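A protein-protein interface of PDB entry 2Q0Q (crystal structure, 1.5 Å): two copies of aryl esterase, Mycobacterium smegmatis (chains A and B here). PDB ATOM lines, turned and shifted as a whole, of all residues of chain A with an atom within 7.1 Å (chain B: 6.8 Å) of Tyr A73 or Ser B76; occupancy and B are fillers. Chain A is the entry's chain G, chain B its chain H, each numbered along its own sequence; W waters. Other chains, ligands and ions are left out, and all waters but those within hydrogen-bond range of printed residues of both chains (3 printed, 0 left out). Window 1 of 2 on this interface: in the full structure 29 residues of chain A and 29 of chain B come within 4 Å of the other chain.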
ATOM      1  N   PHE A   8      23.832  -5.740  12.485  1.00  0.00           N
ATOM      2  CA  PHE A   8      23.449  -4.694  13.422  1.00  0.00           C
ATOM      3  C   PHE A   8      22.845  -3.530  12.653  1.00  0.00           C
ATOM      4  O   PHE A   8      23.501  -2.951  11.787  1.00  0.00           O
ATOM      5  CB  PHE A   8      24.674  -4.233  14.232  1.00  0.00           C
ATOM      6  CG  PHE A   8      24.326  -3.434  15.462  1.00  0.00           C
ATOM      7  CD1 PHE A   8      23.698  -4.051  16.542  1.00  0.00           C
ATOM      8  CD2 PHE A   8      24.629  -2.089  15.553  1.00  0.00           C
ATOM      9  CE1 PHE A   8      23.380  -3.343  17.678  1.00  0.00           C
ATOM     10  CE2 PHE A   8      24.316  -1.373  16.697  1.00  0.00           C
ATOM     11  CZ  PHE A   8      23.677  -2.001  17.757  1.00  0.00           C
ATOM     12  N   GLU A  50      20.424 -11.695  13.691  1.00  0.00           N
ATOM     13  CA  GLU A  50      19.592 -10.508  13.418  1.00  0.00           C
ATOM     14  C   GLU A  50      19.475  -9.611  14.632  1.00  0.00           C
ATOM     15  O   GLU A  50      18.786  -9.945  15.604  1.00  0.00           O
ATOM     16  CB  GLU A  50      18.192 -10.929  12.983  1.00  0.00           C
ATOM     17  CG  GLU A  50      18.219 -11.776  11.720  1.00  0.00           C
ATOM     18  CD  GLU A  50      16.871 -12.359  11.328  1.00  0.00           C
ATOM     19  OE1 GLU A  50      16.050 -12.705  12.218  1.00  0.00           O
ATOM     20  OE2 GLU A  50      16.654 -12.483  10.108  1.00  0.00           O
ATOM     21  N   GLU A  51      20.180  -8.490  14.592  1.00  0.00           N
ATOM     22  CA  GLU A  51      20.060  -7.471  15.625  1.00  0.00           C
ATOM     23  C   GLU A  51      19.679  -6.131  14.989  1.00  0.00           C
ATOM     24  O   GLU A  51      20.439  -5.174  15.025  1.00  0.00           O
ATOM     25  CB  GLU A  51      21.351  -7.369  16.441  1.00  0.00           C
ATOM     26  CG  GLU A  51      21.620  -8.597  17.329  1.00  0.00           C
ATOM     27  CD  GLU A  51      20.851  -8.609  18.627  1.00  0.00           C
ATOM     28  OE1 GLU A  51      20.240  -7.573  19.014  1.00  0.00           O
ATOM     29  OE2 GLU A  51      20.923  -9.655  19.323  1.00  0.00           O
ATOM     30  N   GLY A  52      18.460  -6.075  14.458  1.00  0.00           N
ATOM     31  CA  GLY A  52      17.910  -4.855  13.912  1.00  0.00           C
ATOM     32  C   GLY A  52      16.833  -4.329  14.844  1.00  0.00           C
ATOM     33  O   GLY A  52      15.905  -5.070  15.180  1.00  0.00           O
ATOM     34  N   LEU A  53      16.948  -3.051  15.231  1.00  0.00           N
ATOM     35  CA  LEU A  53      15.965  -2.357  16.067  1.00  0.00           C
ATOM     36  C   LEU A  53      15.401  -1.111  15.367  1.00  0.00           C
ATOM     37  O   LEU A  53      16.135  -0.142  15.113  1.00  0.00           O
ATOM     38  CB  LEU A  53      16.619  -1.928  17.402  1.00  0.00           C
ATOM     39  CG  LEU A  53      15.785  -1.030  18.329  1.00  0.00           C
ATOM     40  CD1 LEU A  53      14.478  -1.713  18.702  1.00  0.00           C
ATOM     41  CD2 LEU A  53      16.610  -0.674  19.559  1.00  0.00           C
ATOM     42  N   ARG A  56      16.523   2.874  15.556  1.00  0.00           N
ATOM     43  CA  ARG A  56      17.864   2.956  16.115  1.00  0.00           C
ATOM     44  C   ARG A  56      18.723   3.979  15.369  1.00  0.00           C
ATOM     45  O   ARG A  56      18.707   4.061  14.124  1.00  0.00           O
ATOM     46  CB  ARG A  56      18.558   1.590  16.031  1.00  0.00           C
ATOM     47  CG  ARG A  56      19.998   1.598  16.532  1.00  0.00           C
ATOM     48  CD  ARG A  56      20.529   0.199  16.600  1.00  0.00           C
ATOM     49  NE  ARG A  56      20.137  -0.475  17.828  1.00  0.00           N
ATOM     50  CZ  ARG A  56      20.107  -1.792  17.975  1.00  0.00           C
ATOM     51  NH1 ARG A  56      20.349  -2.600  16.952  1.00  0.00           N
ATOM     52  NH2 ARG A  56      19.784  -2.293  19.159  1.00  0.00           N
ATOM     53  N   ASP A  65      12.338   7.965  23.110  1.00  0.00           N
ATOM     54  CA  ASP A  65      12.480   6.523  23.314  1.00  0.00           C
ATOM     55  C   ASP A  65      13.905   6.224  23.765  1.00  0.00           C
ATOM     56  O   ASP A  65      14.852   6.443  23.014  1.00  0.00           O
ATOM     57  CB  ASP A  65      12.171   5.797  22.007  1.00  0.00           C
ATOM     58  CG  ASP A  65      12.050   4.304  22.175  1.00  0.00           C
ATOM     59  OD1 ASP A  65      12.663   3.737  23.103  1.00  0.00           O
ATOM     60  OD2 ASP A  65      11.356   3.692  21.344  1.00  0.00           O
ATOM     61  N   PRO A  66      14.067   5.690  24.984  1.00  0.00           N
ATOM     62  CA  PRO A  66      15.406   5.404  25.516  1.00  0.00           C
ATOM     63  C   PRO A  66      16.090   4.168  24.929  1.00  0.00           C
ATOM     64  O   PRO A  66      17.212   3.860  25.318  1.00  0.00           O
ATOM     65  CB  PRO A  66      15.121   5.165  27.008  1.00  0.00           C
ATOM     66  CG  PRO A  66      13.736   4.567  26.986  1.00  0.00           C
ATOM     67  CD  PRO A  66      13.011   5.333  25.955  1.00  0.00           C
ATOM     68  N   ARG A  67      15.413   3.440  24.045  1.00  0.00           N
ATOM     69  CA  ARG A  67      15.944   2.178  23.518  1.00  0.00           C
ATOM     70  C   ARG A  67      16.866   2.293  22.313  1.00  0.00           C
ATOM     71  O   ARG A  67      17.402   1.278  21.864  1.00  0.00           O
ATOM     72  CB  ARG A  67      14.772   1.271  23.134  1.00  0.00           C
ATOM     73  CG  ARG A  67      13.935   0.816  24.359  1.00  0.00           C
ATOM     74  CD  ARG A  67      12.694   0.032  23.916  1.00  0.00           C
ATOM     75  NE  ARG A  67      11.762   0.868  23.149  1.00  0.00           N
ATOM     76  CZ  ARG A  67      10.528   0.498  22.811  1.00  0.00           C
ATOM     77  NH1 ARG A  67      10.055  -0.681  23.186  1.00  0.00           N
ATOM     78  NH2 ARG A  67       9.746   1.321  22.138  1.00  0.00           N
ATOM     79  N   LEU A  68      17.035   3.494  21.758  1.00  0.00           N
ATOM     80  CA  LEU A  68      17.451   3.607  20.354  1.00  0.00           C
ATOM     81  C   LEU A  68      18.904   3.983  20.048  1.00  0.00           C
ATOM     82  O   LEU A  68      19.256   4.107  18.876  1.00  0.00           O
ATOM     83  CB  LEU A  68      16.493   4.576  19.652  1.00  0.00           C
ATOM     84  CG  LEU A  68      15.010   4.213  19.801  1.00  0.00           C
ATOM     85  CD1 LEU A  68      14.142   5.254  19.058  1.00  0.00           C
ATOM     86  CD2 LEU A  68      14.754   2.789  19.323  1.00  0.00           C
ATOM     87  N   ASN A  69      19.741   4.177  21.067  1.00  0.00           N
ATOM     88  CA  ASN A  69      21.153   4.510  20.864  1.00  0.00           C
ATOM     89  C   ASN A  69      21.961   3.252  20.526  1.00  0.00           C
ATOM     90  O   ASN A  69      22.219   2.399  21.417  1.00  0.00           O
ATOM     91  CB  ASN A  69      21.697   5.188  22.119  1.00  0.00           C
ATOM     92  CG  ASN A  69      23.140   5.670  21.970  1.00  0.00           C
ATOM     93  OD1 ASN A  69      23.959   5.045  21.291  1.00  0.00           O
ATOM     94  ND2 ASN A  69      23.452   6.776  22.622  1.00  0.00           N
ATOM     95  N   GLY A  70      22.373   3.128  19.258  1.00  0.00           N
ATOM     96  CA  GLY A  70      23.052   1.915  18.800  1.00  0.00           C
ATOM     97  C   GLY A  70      24.312   1.626  19.596  1.00  0.00           C
ATOM     98  O   GLY A  70      24.525   0.497  20.054  1.00  0.00           O
ATOM     99  N   ALA A  71      25.109   2.671  19.862  1.00  0.00           N
ATOM    100  CA  ALA A  71      26.392   2.508  20.572  1.00  0.00           C
ATOM    101  C   ALA A  71      26.215   2.126  22.034  1.00  0.00           C
ATOM    102  O   ALA A  71      27.161   1.650  22.655  1.00  0.00           O
ATOM    103  CB  ALA A  71      27.207   3.783  20.487  1.00  0.00           C
ATOM    104  N   SER A  72      25.020   2.340  22.564  1.00  0.00           N
ATOM    105  CA  SER A  72      24.762   1.965  23.965  1.00  0.00           C
ATOM    106  C   SER A  72      24.650   0.455  24.068  1.00  0.00           C
ATOM    107  O   SER A  72      24.951  -0.123  25.115  1.00  0.00           O
ATOM    108  CB  SER A  72      23.461   2.592  24.498  1.00  0.00           C
ATOM    109  OG  SER A  72      23.587   3.990  24.656  1.00  0.00           O
ATOM    110  N   TYR A  73      24.196  -0.166  22.990  1.00  0.00           N
ATOM    111  CA  TYR A  73      23.828  -1.568  22.967  1.00  0.00           C
ATOM    112  C   TYR A  73      24.934  -2.438  22.363  1.00  0.00           C
ATOM    113  O   TYR A  73      25.141  -3.580  22.775  1.00  0.00           O
ATOM    114  CB  TYR A  73      22.547  -1.667  22.163  1.00  0.00           C
ATOM    115  CG  TYR A  73      21.820  -2.985  22.076  1.00  0.00           C
ATOM    116  CD1 TYR A  73      22.121  -3.903  21.091  1.00  0.00           C
ATOM    117  CD2 TYR A  73      20.731  -3.254  22.897  1.00  0.00           C
ATOM    118  CE1 TYR A  73      21.411  -5.095  20.962  1.00  0.00           C
ATOM    119  CE2 TYR A  73      20.014  -4.442  22.786  1.00  0.00           C
ATOM    120  CZ  TYR A  73      20.351  -5.357  21.807  1.00  0.00           C
ATOM    121  OH  TYR A  73      19.632  -6.531  21.659  1.00  0.00           O
ATOM    122  N   LEU A  74      25.652  -1.910  21.372  1.00  0.00           N
ATOM    123  CA  LEU A  74      26.495  -2.785  20.566  1.00  0.00           C
ATOM    124  C   LEU A  74      27.575  -3.553  21.355  1.00  0.00           C
ATOM    125  O   LEU A  74      27.743  -4.738  21.142  1.00  0.00           O
ATOM    126  CB  LEU A  74      27.126  -2.029  19.387  1.00  0.00           C
ATOM    127  CG  LEU A  74      28.023  -2.856  18.460  1.00  0.00           C
ATOM    128  CD1 LEU A  74      27.266  -4.018  17.853  1.00  0.00           C
ATOM    129  CD2 LEU A  74      28.608  -1.957  17.358  1.00  0.00           C
ATOM    130  N   PRO A  75      28.315  -2.885  22.257  1.00  0.00           N
ATOM    131  CA  PRO A  75      29.361  -3.634  22.988  1.00  0.00           C
ATOM    132  C   PRO A  75      28.817  -4.826  23.752  1.00  0.00           C
ATOM    133  O   PRO A  75      29.439  -5.892  23.776  1.00  0.00           O
ATOM    134  CB  PRO A  75      29.929  -2.584  23.941  1.00  0.00           C
ATOM    135  CG  PRO A  75      29.629  -1.257  23.239  1.00  0.00           C
ATOM    136  CD  PRO A  75      28.279  -1.471  22.667  1.00  0.00           C
ATOM    137  N   SER A  76      27.664  -4.648  24.389  1.00  0.00           N
ATOM    138  CA  SER A  76      26.985  -5.760  25.067  1.00  0.00           C
ATOM    139  C   SER A  76      26.563  -6.849  24.089  1.00  0.00           C
ATOM    140  O   SER A  76      26.698  -8.047  24.353  1.00  0.00           O
ATOM    141  CB  SER A  76      25.762  -5.261  25.818  1.00  0.00           C
ATOM    142  OG  SER A  76      26.134  -4.430  26.896  1.00  0.00           O
ATOM    143  N   CYS A  77      26.079  -6.421  22.934  1.00  0.00           N
ATOM    144  CA  CYS A  77      25.626  -7.334  21.887  1.00  0.00           C
ATOM    145  C   CYS A  77      26.810  -8.165  21.340  1.00  0.00           C
ATOM    146  O   CYS A  77      26.708  -9.384  21.206  1.00  0.00           O
ATOM    147  CB  CYS A  77      24.930  -6.525  20.789  1.00  0.00           C
ATOM    148  SG  CYS A  77      24.147  -7.422  19.457  1.00  0.00           S
ATOM    149  N   LEU A  78      27.946  -7.512  21.080  1.00  0.00           N
ATOM    150  CA  LEU A  78      29.137  -8.200  20.588  1.00  0.00           C
ATOM    151  C   LEU A  78      29.596  -9.292  21.551  1.00  0.00           C
ATOM    152  O   LEU A  78      29.933 -10.398  21.144  1.00  0.00           O
ATOM    153  CB  LEU A  78      30.281  -7.195  20.343  1.00  0.00           C
ATOM    154  CG  LEU A  78      30.154  -6.245  19.137  1.00  0.00           C
ATOM    155  CD1 LEU A  78      31.181  -5.110  19.233  1.00  0.00           C
ATOM    156  CD2 LEU A  78      30.285  -6.997  17.816  1.00  0.00           C
ATOM    157  N   ALA A  79      29.578  -8.968  22.838  1.00  0.00           N
ATOM    158  CA  ALA A  79      30.081  -9.910  23.844  1.00  0.00           C
ATOM    159  C   ALA A  79      29.116 -11.096  24.061  1.00  0.00           C
ATOM    160  O   ALA A  79      29.535 -12.177  24.466  1.00  0.00           O
ATOM    161  CB  ALA A  79      30.342  -9.189  25.153  1.00  0.00           C
ATOM    162  N   THR A  80      27.834 -10.832  23.847  1.00  0.00           N
ATOM    163  CA  THR A  80      26.754 -11.824  23.881  1.00  0.00           C
ATOM    164  C   THR A  80      26.940 -12.896  22.778  1.00  0.00           C
ATOM    165  O   THR A  80      26.696 -14.083  23.000  1.00  0.00           O
ATOM    166  CB  THR A  80      25.386 -11.107  23.677  1.00  0.00           C
ATOM    167  OG1 THR A  80      25.085 -10.287  24.808  1.00  0.00           O
ATOM    168  CG2 THR A  80      24.243 -12.075  23.401  1.00  0.00           C
ATOM    169  N   HIS A  81      27.346 -12.462  21.586  1.00  0.00           N
ATOM    170  CA  HIS A  81      27.314 -13.328  20.414  1.00  0.00           C
ATOM    171  C   HIS A  81      28.669 -13.882  19.973  1.00  0.00           C
ATOM    172  O   HIS A  81      28.719 -14.664  18.997  1.00  0.00           O
ATOM    173  CB  HIS A  81      26.634 -12.610  19.231  1.00  0.00           C
ATOM    174  CG  HIS A  81      25.189 -12.310  19.474  1.00  0.00           C
ATOM    175  ND1 HIS A  81      24.254 -13.298  19.708  1.00  0.00           N
ATOM    176  CD2 HIS A  81      24.514 -11.136  19.508  1.00  0.00           C
ATOM    177  CE1 HIS A  81      23.068 -12.743  19.892  1.00  0.00           C
ATOM    178  NE2 HIS A  81      23.200 -11.434  19.782  1.00  0.00           N
ATOM    179  N   LEU A 114      30.800   3.017  16.493  1.00  0.00           N
ATOM    180  CA  LEU A 114      30.371   1.623  16.335  1.00  0.00           C
ATOM    181  C   LEU A 114      31.495   0.732  15.743  1.00  0.00           C
ATOM    182  O   LEU A 114      31.761  -0.384  16.235  1.00  0.00           O
ATOM    183  CB  LEU A 114      29.098   1.563  15.472  1.00  0.00           C
ATOM    184  CG  LEU A 114      27.858   2.299  16.022  1.00  0.00           C
ATOM    185  CD1 LEU A 114      26.690   2.213  15.072  1.00  0.00           C
ATOM    186  CD2 LEU A 114      27.438   1.749  17.344  1.00  0.00           C
ATOM    187  N   GLN A 117      34.028   0.132  18.424  1.00  0.00           N
ATOM    188  CA  GLN A 117      33.481  -0.922  19.320  1.00  0.00           C
ATOM    189  C   GLN A 117      33.667  -2.349  18.747  1.00  0.00           C
ATOM    190  O   GLN A 117      33.973  -3.302  19.489  1.00  0.00           O
ATOM    191  CB  GLN A 117      32.008  -0.656  19.631  1.00  0.00           C
ATOM    192  CG  GLN A 117      31.727   0.573  20.482  1.00  0.00           C
ATOM    193  CD  GLN A 117      30.242   0.863  20.674  1.00  0.00           C
ATOM    194  OE1 GLN A 117      29.393   0.372  19.928  1.00  0.00           O
ATOM    195  NE2 GLN A 117      29.921   1.664  21.711  1.00  0.00           N
ATOM    196  N   GLU B  51      20.277 -14.844  24.139  1.00  0.00           N
ATOM    197  CA  GLU B  51      20.782 -13.539  24.583  1.00  0.00           C
ATOM    198  C   GLU B  51      21.385 -13.674  25.978  1.00  0.00           C
ATOM    199  O   GLU B  51      20.875 -13.134  26.963  1.00  0.00           O
ATOM    200  CB  GLU B  51      19.672 -12.475  24.539  1.00  0.00           C
ATOM    201  CG  GLU B  51      19.226 -12.076  23.084  1.00  0.00           C
ATOM    202  CD  GLU B  51      20.082 -10.973  22.462  1.00  0.00           C
ATOM    203  OE1 GLU B  51      21.069 -10.528  23.070  1.00  0.00           O
ATOM    204  OE2 GLU B  51      19.769 -10.523  21.332  1.00  0.00           O
ATOM    205  N   ALA B  71      19.035  -4.848  32.752  1.00  0.00           N
ATOM    206  CA  ALA B  71      17.886  -3.999  32.574  1.00  0.00           C
ATOM    207  C   ALA B  71      18.165  -2.834  31.605  1.00  0.00           C
ATOM    208  O   ALA B  71      17.230  -2.250  31.047  1.00  0.00           O
ATOM    209  CB  ALA B  71      17.417  -3.454  33.930  1.00  0.00           C
ATOM    210  N   SER B  72      19.434  -2.495  31.427  1.00  0.00           N
ATOM    211  CA  SER B  72      19.787  -1.436  30.497  1.00  0.00           C
ATOM    212  C   SER B  72      19.595  -1.939  29.088  1.00  0.00           C
ATOM    213  O   SER B  72      19.307  -1.153  28.196  1.00  0.00           O
ATOM    214  CB  SER B  72      21.234  -1.002  30.671  1.00  0.00           C
ATOM    215  OG  SER B  72      21.433  -0.438  31.945  1.00  0.00           O
ATOM    216  N   TYR B  73      19.789  -3.243  28.891  1.00  0.00           N
ATOM    217  CA  TYR B  73      19.756  -3.892  27.550  1.00  0.00           C
ATOM    218  C   TYR B  73      18.415  -4.508  27.149  1.00  0.00           C
ATOM    219  O   TYR B  73      18.059  -4.524  25.961  1.00  0.00           O
ATOM    220  CB  TYR B  73      20.774  -5.033  27.592  1.00  0.00           C
ATOM    221  CG  TYR B  73      21.172  -5.750  26.294  1.00  0.00           C
ATOM    222  CD1 TYR B  73      20.497  -6.892  25.857  1.00  0.00           C
ATOM    223  CD2 TYR B  73      22.291  -5.331  25.552  1.00  0.00           C
ATOM    224  CE1 TYR B  73      20.916  -7.595  24.706  1.00  0.00           C
ATOM    225  CE2 TYR B  73      22.712  -6.031  24.413  1.00  0.00           C
ATOM    226  CZ  TYR B  73      22.029  -7.157  23.992  1.00  0.00           C
ATOM    227  OH  TYR B  73      22.451  -7.839  22.843  1.00  0.00           O
ATOM    228  N   LEU B  74      17.705  -5.074  28.121  1.00  0.00           N
ATOM    229  CA  LEU B  74      16.550  -5.908  27.822  1.00  0.00           C
ATOM    230  C   LEU B  74      15.457  -5.209  26.967  1.00  0.00           C
ATOM    231  O   LEU B  74      14.963  -5.798  25.995  1.00  0.00           O
ATOM    232  CB  LEU B  74      15.968  -6.518  29.104  1.00  0.00           C
ATOM    233  CG  LEU B  74      14.831  -7.492  28.825  1.00  0.00           C
ATOM    234  CD1 LEU B  74      15.222  -8.607  27.917  1.00  0.00           C
ATOM    235  CD2 LEU B  74      14.304  -8.039  30.121  1.00  0.00           C
ATOM    236  N   PRO B  75      15.037  -3.966  27.325  1.00  0.00           N
ATOM    237  CA  PRO B  75      13.990  -3.304  26.524  1.00  0.00           C
ATOM    238  C   PRO B  75      14.336  -3.200  25.013  1.00  0.00           C
ATOM    239  O   PRO B  75      13.476  -3.431  24.147  1.00  0.00           O
ATOM    240  CB  PRO B  75      13.889  -1.913  27.179  1.00  0.00           C
ATOM    241  CG  PRO B  75      14.228  -2.195  28.603  1.00  0.00           C
ATOM    242  CD  PRO B  75      15.406  -3.137  28.489  1.00  0.00           C
ATOM    243  N   SER B  76      15.574  -2.834  24.722  1.00  0.00           N
ATOM    244  CA  SER B  76      16.044  -2.772  23.318  1.00  0.00           C
ATOM    245  C   SER B  76      16.075  -4.164  22.673  1.00  0.00           C
ATOM    246  O   SER B  76      15.711  -4.341  21.491  1.00  0.00           O
ATOM    247  CB  SER B  76      17.438  -2.134  23.238  1.00  0.00           C
ATOM    248  OG  SER B  76      17.461  -0.828  23.818  1.00  0.00           O
ATOM    249  N   CYS B  77      16.504  -5.153  23.461  1.00  0.00           N
ATOM    250  CA  CYS B  77      16.508  -6.552  23.041  1.00  0.00           C
ATOM    251  C   CYS B  77      15.090  -7.070  22.674  1.00  0.00           C
ATOM    252  O   CYS B  77      14.899  -7.674  21.615  1.00  0.00           O
ATOM    253  CB  CYS B  77      17.131  -7.395  24.157  1.00  0.00           C
ATOM    254  SG  CYS B  77      17.511  -9.048  23.695  1.00  0.00           S
ATOM    255  N   LEU B  78      14.098  -6.773  23.515  1.00  0.00           N
ATOM    256  CA  LEU B  78      12.741  -7.238  23.299  1.00  0.00           C
ATOM    257  C   LEU B  78      12.159  -6.628  22.012  1.00  0.00           C
ATOM    258  O   LEU B  78      11.608  -7.335  21.172  1.00  0.00           O
ATOM    259  CB  LEU B  78      11.843  -6.870  24.481  1.00  0.00           C
ATOM    260  CG  LEU B  78      12.107  -7.554  25.829  1.00  0.00           C
ATOM    261  CD1 LEU B  78      11.324  -6.851  26.935  1.00  0.00           C
ATOM    262  CD2 LEU B  78      11.721  -9.029  25.727  1.00  0.00           C
ATOM    263  N   ALA B  79      12.287  -5.313  21.863  1.00  0.00           N
ATOM    264  CA  ALA B  79      11.823  -4.639  20.636  1.00  0.00           C
ATOM    265  C   ALA B  79      12.554  -5.165  19.357  1.00  0.00           C
ATOM    266  O   ALA B  79      11.969  -5.193  18.270  1.00  0.00           O
ATOM    267  CB  ALA B  79      12.000  -3.137  20.786  1.00  0.00           C
ATOM    268  N   THR B  80      13.824  -5.538  19.501  1.00  0.00           N
ATOM    269  CA  THR B  80      14.648  -6.094  18.419  1.00  0.00           C
ATOM    270  C   THR B  80      14.112  -7.416  17.903  1.00  0.00           C
ATOM    271  O   THR B  80      14.200  -7.697  16.709  1.00  0.00           O
ATOM    272  CB  THR B  80      16.118  -6.326  18.901  1.00  0.00           C
ATOM    273  OG1 THR B  80      16.767  -5.072  19.100  1.00  0.00           O
ATOM    274  CG2 THR B  80      16.935  -7.175  17.903  1.00  0.00           C
ATOM    275  N   HIS B  81      13.556  -8.225  18.808  1.00  0.00           N
ATOM    276  CA  HIS B  81      13.214  -9.611  18.491  1.00  0.00           C
ATOM    277  C   HIS B  81      11.716  -9.844  18.347  1.00  0.00           C
ATOM    278  O   HIS B  81      11.311 -10.958  18.068  1.00  0.00           O
ATOM    279  CB  HIS B  81      13.854 -10.577  19.510  1.00  0.00           C
ATOM    280  CG  HIS B  81      15.348 -10.647  19.401  1.00  0.00           C
ATOM    281  ND1 HIS B  81      15.989 -11.082  18.261  1.00  0.00           N
ATOM    282  CD2 HIS B  81      16.329 -10.300  20.273  1.00  0.00           C
ATOM    283  CE1 HIS B  81      17.298 -11.027  18.444  1.00  0.00           C
ATOM    284  NE2 HIS B  81      17.531 -10.554  19.656  1.00  0.00           N
HETATM  285  O   HOH W   1      19.269  -4.943  18.428  1.00  0.00           O
HETATM  286  O   HOH W   2      22.377 -10.307  25.618  1.00  0.00           O
HETATM  287  O   HOH W   3      10.855  -2.999  24.726  1.00  0.00           O
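The side-chain carboxylate (OE2) of Glu A51 sits close to the side-chain carboxylate (OE2) of Glu B51 (2.5 Å).
OG of Ser B76 sits at hydrogen-bond distance from O of Arg A67 (2.9 Å).
The side-chain hydroxyl (OH) of Tyr B73 lies within hydrogen-bond range of the side-chain hydroxyl (OH) of Tyr A73 (3.3 Å).
The backbone carbonyl oxygen (O) of Thr B80 lies close to the backbone carbonyl oxygen (O) of Gly A52, at 3.5 Å.
OE1 of Glu A51 sits at hydrogen-bond distance from OH of Tyr A73, at 2.9 Å.
The side-chain carboxylate of Glu A51 sits at hydrogen-bond distance from a ring nitrogen (NE2) of His A81 (2.9 Å).
The backbone carbonyl oxygen (O) of Ser A76 lies within hydrogen-bond range of the side-chain hydroxyl (OG1) of Thr A80 (2.8 Å).
OE1 of Glu B51 lies within hydrogen-bond range of OH of Tyr B73.
OE2 of Glu B51 sits close to SG of Cys B77, 3.6 Å away.
The side-chain hydroxyl (OG1) of Thr B80 lies within hydrogen-bond range of the backbone carbonyl oxygen (O) of Ser B76 (2.7 Å).
CE1 of His B81 touches O of Glu A50 (3.4 Å).
Glu A51 touches His B81.
CB of Leu A53 touches OG1 of Thr B80, at 3.6 Å.
Pro B75 touches Arg A67.
Arg A67 touches Ala B79.
Tyr A73 touches Ser B76.
Ser A76 touches Tyr B73.
CA of Cys A77 touches OH of Tyr B73, 3.4 Å away.
Thr A80 touches Glu B51 (CG2 to OE1, 3.5 Å).
His A81 touches Glu B51 (NE2 to OE2, 3.9 Å).
Of the printed residues of chain B, Glu A50 touches His B81 (3.4 Å).
Of the printed residues of chain B, Tyr A73 touches Tyr B73, Ser B76 and Cys B77.
Pro A75 touches none of the printed residues of chain B.
Printed residues of chain B within 4 Å of Cys A77: Tyr B73 (3.4 Å).
Ala B71 touches none of the printed residues of chain A.
Ser B76 touches two residues of chain A.
The nearest printed residue of chain B that does not touch Tyr A73 is Glu B51 (4.01 Å).
The nearest printed residue of chain B that does not touch Ser A76 is Glu B51 (6.3 Å).
Printed residues of chain A that touch a printed residue of chain B: Glu A50, Glu A51, Gly A52, Leu A53, Arg A67, Tyr A73, Ser A76, Cys A77, Thr A80 and His A81.
Hydrophobic or aromatic side chains of chain A within 4 Å of the printed part of chain B: Leu A53, Tyr A73 and His A81.
Glu A51 touches His B81, and with the chains exchanged His A81 touches Glu B51.
Tyr B73 touches its own counterpart, Tyr A73.
Tyr A73 touches Ser B76, and with the chains exchanged Ser A76 touches Tyr B73.
Tyr A73 touches Cys B77, and with the chains exchanged Cys A77 touches Tyr B73.
Water W1 lies within hydrogen-bond range of OG1 of Thr B80, NH2 of Arg A56 and OE1 of Glu A51.
Water W3 lies within hydrogen-bond range of O of Pro B75 (2.7 Å) and NH1 of Arg A67 (2.9 Å).
Water W2 lies within hydrogen-bond range of OG1 of Thr A80 (2.8 Å) and OE1 of Glu B51 (2.9 Å).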
